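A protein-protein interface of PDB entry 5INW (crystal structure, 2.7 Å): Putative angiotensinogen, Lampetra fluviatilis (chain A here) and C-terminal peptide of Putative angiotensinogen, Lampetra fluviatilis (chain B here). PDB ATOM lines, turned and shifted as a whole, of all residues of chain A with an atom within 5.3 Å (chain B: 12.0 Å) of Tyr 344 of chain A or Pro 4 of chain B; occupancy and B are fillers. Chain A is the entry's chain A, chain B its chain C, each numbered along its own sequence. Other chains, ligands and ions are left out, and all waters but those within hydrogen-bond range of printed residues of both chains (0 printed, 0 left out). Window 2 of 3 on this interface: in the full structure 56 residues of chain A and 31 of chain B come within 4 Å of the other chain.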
ATOM      1  N   ARG A 282     -11.230  17.716  10.421  1.00  0.00           N
ATOM      2  CA  ARG A 282     -11.525  19.111  10.327  1.00  0.00           C
ATOM      3  C   ARG A 282     -13.026  19.153  10.093  1.00  0.00           C
ATOM      4  O   ARG A 282     -13.477  18.886   8.974  1.00  0.00           O
ATOM      5  CB  ARG A 282     -10.722  19.778   9.194  1.00  0.00           C
ATOM      6  CG  ARG A 282     -10.372  21.221   9.519  1.00  0.00           C
ATOM      7  CD  ARG A 282      -9.955  22.082   8.331  1.00  0.00           C
ATOM      8  NE  ARG A 282     -11.096  22.465   7.502  1.00  0.00           N
ATOM      9  CZ  ARG A 282     -11.078  23.380   6.534  1.00  0.00           C
ATOM     10  NH1 ARG A 282      -9.965  24.045   6.236  1.00  0.00           N
ATOM     11  NH2 ARG A 282     -12.195  23.633   5.850  1.00  0.00           N
ATOM     12  N   ALA A 283     -13.800  19.460  11.140  1.00  0.00           N
ATOM     13  CA  ALA A 283     -15.244  19.688  10.972  1.00  0.00           C
ATOM     14  C   ALA A 283     -15.775  20.880  11.772  1.00  0.00           C
ATOM     15  O   ALA A 283     -15.060  21.445  12.604  1.00  0.00           O
ATOM     16  CB  ALA A 283     -16.006  18.423  11.301  1.00  0.00           C
ATOM     17  N   LYS A 284     -17.029  21.240  11.492  1.00  0.00           N
ATOM     18  CA  LYS A 284     -17.745  22.335  12.163  1.00  0.00           C
ATOM     19  C   LYS A 284     -18.368  21.876  13.498  1.00  0.00           C
ATOM     20  O   LYS A 284     -19.494  21.387  13.532  1.00  0.00           O
ATOM     21  CB  LYS A 284     -18.835  22.886  11.235  1.00  0.00           C
ATOM     22  CG  LYS A 284     -18.306  23.322   9.884  1.00  0.00           C
ATOM     23  CD  LYS A 284     -19.375  23.956   9.019  1.00  0.00           C
ATOM     24  CE  LYS A 284     -18.756  24.303   7.689  1.00  0.00           C
ATOM     25  NZ  LYS A 284     -19.702  25.051   6.832  1.00  0.00           N
ATOM     26  N   TYR A 287     -17.583  24.452  20.251  1.00  0.00           N
ATOM     27  CA  TYR A 287     -16.597  24.366  21.326  1.00  0.00           C
ATOM     28  C   TYR A 287     -16.624  25.675  22.091  1.00  0.00           C
ATOM     29  O   TYR A 287     -17.234  26.642  21.653  1.00  0.00           O
ATOM     30  CB  TYR A 287     -15.197  24.112  20.768  1.00  0.00           C
ATOM     31  CG  TYR A 287     -14.648  25.243  19.927  1.00  0.00           C
ATOM     32  CD1 TYR A 287     -15.247  25.555  18.710  1.00  0.00           C
ATOM     33  CD2 TYR A 287     -13.545  26.015  20.353  1.00  0.00           C
ATOM     34  CE1 TYR A 287     -14.791  26.609  17.942  1.00  0.00           C
ATOM     35  CE2 TYR A 287     -13.075  27.064  19.582  1.00  0.00           C
ATOM     36  CZ  TYR A 287     -13.695  27.357  18.375  1.00  0.00           C
ATOM     37  OH  TYR A 287     -13.245  28.384  17.569  1.00  0.00           O
ATOM     38  N   ASN A 342     -19.808  27.413  14.286  1.00  0.00           N
ATOM     39  CA  ASN A 342     -19.615  26.608  13.076  1.00  0.00           C
ATOM     40  C   ASN A 342     -18.813  27.361  12.028  1.00  0.00           C
ATOM     41  O   ASN A 342     -19.300  27.736  10.953  1.00  0.00           O
ATOM     42  CB  ASN A 342     -20.940  26.056  12.546  1.00  0.00           C
ATOM     43  CG  ASN A 342     -21.631  25.155  13.564  1.00  0.00           C
ATOM     44  OD1 ASN A 342     -22.716  25.464  14.034  1.00  0.00           O
ATOM     45  ND2 ASN A 342     -20.994  24.058  13.930  1.00  0.00           N
ATOM     46  N   HIS A 343     -17.578  27.627  12.452  1.00  0.00           N
ATOM     47  CA  HIS A 343     -16.408  27.600  11.612  1.00  0.00           C
ATOM     48  C   HIS A 343     -15.763  26.250  11.913  1.00  0.00           C
ATOM     49  O   HIS A 343     -15.896  25.716  13.006  1.00  0.00           O
ATOM     50  CB  HIS A 343     -15.452  28.761  11.947  1.00  0.00           C
ATOM     51  CG  HIS A 343     -16.142  30.079  12.068  1.00  0.00           C
ATOM     52  ND1 HIS A 343     -16.372  30.900  10.986  1.00  0.00           N
ATOM     53  CD2 HIS A 343     -16.701  30.694  13.137  1.00  0.00           C
ATOM     54  CE1 HIS A 343     -17.017  31.980  11.387  1.00  0.00           C
ATOM     55  NE2 HIS A 343     -17.227  31.882  12.689  1.00  0.00           N
ATOM     56  N   TYR A 344     -15.037  25.722  10.937  1.00  0.00           N
ATOM     57  CA  TYR A 344     -14.323  24.463  11.073  1.00  0.00           C
ATOM     58  C   TYR A 344     -13.319  24.459  12.246  1.00  0.00           C
ATOM     59  O   TYR A 344     -12.650  25.460  12.526  1.00  0.00           O
ATOM     60  CB  TYR A 344     -13.573  24.129   9.770  1.00  0.00           C
ATOM     61  CG  TYR A 344     -14.415  23.634   8.578  1.00  0.00           C
ATOM     62  CD1 TYR A 344     -14.671  22.276   8.391  1.00  0.00           C
ATOM     63  CD2 TYR A 344     -14.882  24.519   7.605  1.00  0.00           C
ATOM     64  CE1 TYR A 344     -15.399  21.817   7.304  1.00  0.00           C
ATOM     65  CE2 TYR A 344     -15.609  24.064   6.510  1.00  0.00           C
ATOM     66  CZ  TYR A 344     -15.863  22.709   6.363  1.00  0.00           C
ATOM     67  OH  TYR A 344     -16.580  22.266   5.281  1.00  0.00           O
ATOM     68  N   VAL A 345     -13.202  23.305  12.889  1.00  0.00           N
ATOM     69  CA  VAL A 345     -12.309  23.093  14.026  1.00  0.00           C
ATOM     70  C   VAL A 345     -11.346  21.941  13.738  1.00  0.00           C
ATOM     71  O   VAL A 345     -11.701  20.991  13.008  1.00  0.00           O
ATOM     72  CB  VAL A 345     -13.123  22.738  15.280  1.00  0.00           C
ATOM     73  CG1 VAL A 345     -12.212  22.558  16.482  1.00  0.00           C
ATOM     74  CG2 VAL A 345     -14.157  23.824  15.548  1.00  0.00           C
ATOM     75  N   GLN A 346     -10.155  22.016  14.325  1.00  0.00           N
ATOM     76  CA  GLN A 346      -9.153  20.961  14.221  1.00  0.00           C
ATOM     77  C   GLN A 346      -9.235  20.042  15.422  1.00  0.00           C
ATOM     78  O   GLN A 346      -8.808  20.405  16.512  1.00  0.00           O
ATOM     79  CB  GLN A 346      -7.761  21.579  14.170  1.00  0.00           C
ATOM     80  CG  GLN A 346      -7.499  22.419  12.939  1.00  0.00           C
ATOM     81  CD  GLN A 346      -7.348  21.577  11.694  1.00  0.00           C
ATOM     82  OE1 GLN A 346      -7.525  20.345  11.742  1.00  0.00           O
ATOM     83  NE2 GLN A 346      -7.025  22.221  10.564  1.00  0.00           N
ATOM     84  N   PRO B   4      -7.925  27.373  15.350  1.00  0.00           N
ATOM     85  CA  PRO B   4      -9.045  26.890  16.141  1.00  0.00           C
ATOM     86  C   PRO B   4      -8.959  25.366  16.326  1.00  0.00           C
ATOM     87  O   PRO B   4      -9.277  24.595  15.410  1.00  0.00           O
ATOM     88  CB  PRO B   4     -10.259  27.307  15.315  1.00  0.00           C
ATOM     89  CG  PRO B   4      -9.775  27.248  13.913  1.00  0.00           C
ATOM     90  CD  PRO B   4      -8.283  27.525  13.927  1.00  0.00           C
ATOM     91  N   THR B   5      -8.545  24.960  17.529  1.00  0.00           N
ATOM     92  CA  THR B   5      -7.945  23.640  17.769  1.00  0.00           C
ATOM     93  C   THR B   5      -8.388  22.990  19.088  1.00  0.00           C
ATOM     94  O   THR B   5      -8.317  23.601  20.167  1.00  0.00           O
ATOM     95  CB  THR B   5      -6.398  23.755  17.754  1.00  0.00           C
ATOM     96  OG1 THR B   5      -5.983  24.159  16.448  1.00  0.00           O
ATOM     97  CG2 THR B   5      -5.695  22.435  18.115  1.00  0.00           C
ATOM     98  N   VAL B   6      -8.820  21.727  18.989  1.00  0.00           N
ATOM     99  CA  VAL B   6      -9.185  20.918  20.153  1.00  0.00           C
ATOM    100  C   VAL B   6      -8.378  19.632  20.114  1.00  0.00           C
ATOM    101  O   VAL B   6      -8.554  18.822  19.191  1.00  0.00           O
ATOM    102  CB  VAL B   6     -10.688  20.581  20.163  1.00  0.00           C
ATOM    103  CG1 VAL B   6     -11.100  20.022  21.527  1.00  0.00           C
ATOM    104  CG2 VAL B   6     -11.513  21.812  19.807  1.00  0.00           C
ATOM    105  N   THR B   7      -7.479  19.463  21.091  1.00  0.00           N
ATOM    106  CA  THR B   7      -6.684  18.240  21.173  1.00  0.00           C
ATOM    107  C   THR B   7      -6.968  17.547  22.498  1.00  0.00           C
ATOM    108  O   THR B   7      -6.697  18.042  23.564  1.00  0.00           O
ATOM    109  CB  THR B   7      -5.181  18.479  20.979  1.00  0.00           C
ATOM    110  OG1 THR B   7      -4.686  19.163  22.128  1.00  0.00           O
ATOM    111  CG2 THR B   7      -4.908  19.308  19.709  1.00  0.00           C
ATOM    112  N   VAL B   8      -7.567  16.381  22.398  1.00  0.00           N
ATOM    113  CA  VAL B   8      -7.883  15.591  23.543  1.00  0.00           C
ATOM    114  C   VAL B   8      -6.659  14.702  23.683  1.00  0.00           C
ATOM    115  O   VAL B   8      -6.636  13.584  23.165  1.00  0.00           O
ATOM    116  CB  VAL B   8      -9.203  14.809  23.321  1.00  0.00           C
ATOM    117  CG1 VAL B   8      -9.637  14.066  24.596  1.00  0.00           C
ATOM    118  CG2 VAL B   8     -10.300  15.767  22.834  1.00  0.00           C
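O of Ala 283 of chain A is in hydrogen-bond range of N of Val 345 of chain A, at 2.6 Å.
Of the 9 printed residues of chain A, 4 touch a printed residue of chain B.
Printed residues of chain A that touch a printed residue of chain B: Tyr 287, Tyr 344, Val 345 and Gln 346.
Hydrophobic or aromatic side chains of chain A that line the printed part of chain B: Tyr 287 and Val 345.
Along chain A the printed residues that touch a printed residue of chain B span positions 287 to 346.
Hydrophobic or aromatic side chains of chain B that line the printed part of chain A: Pro 4 and Val 6.
Among the printed residues, 7 pairs touch across the chains.
Among the printed residues, no Asp or Glu carboxylate lies within 4 Å of a Lys or Arg side-chain nitrogen of the other chain.
The backbone NH (N) of Val 6 of chain B sits at hydrogen-bond distance from the backbone carbonyl oxygen (O) of Gln 346 of chain A, at 2.8 Å.
The backbone NH (N) of Gln 346 of chain A sits at hydrogen-bond distance from the backbone carbonyl oxygen (O) of Pro 4 of chain B (2.9 Å).
Pro 4 of chain B touches Tyr 287 of chain A.
Pro 4 of chain B touches Tyr 344 of chain A (CG to O, 3.7 Å).
Val 345 of chain A touches Pro 4 of chain B (CA to O, 3.7 Å).
Val 6 of chain B touches Val 345 of chain A.
CA of Thr 5 of chain B touches O of Gln 346 of chain A, at 3.6 Å.
No residue of chain B comes within 4 Å of Arg 282 of chain A.
No residue of chain B comes within 4 Å of Ala 283 of chain A.
Printed residues of chain B within 4 Å of Tyr 287 of chain A: Pro 4 (3.9 Å).
Asn 342 of chain A touches none of the printed residues of chain B.
No residue of chain B comes within 4 Å of His 343 of chain A.
Val 345 of chain A touches just these residues of chain B: Pro 4 and Val 6.
Gln 346 of chain A touches just these residues of chain B: Pro 4 (2.9 Å), Thr 5 (3.6 Å) and Val 6 (2.8 Å).
Pro 4 of chain B touches just these residues of chain A: Tyr 287, Tyr 344, Val 345 and Gln 346.
Of the printed residues of chain A, Thr 5 of chain B touches Gln 346 (3.6 Å).
Of the printed residues of chain A, Val 6 of chain B touches Val 345 and Gln 346.
Thr 7 of chain B touches none of the printed residues of chain A.
The nearest residue of chain B that does not touch Tyr 344 of chain A is Thr 5 of chain B (6.5 Å).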
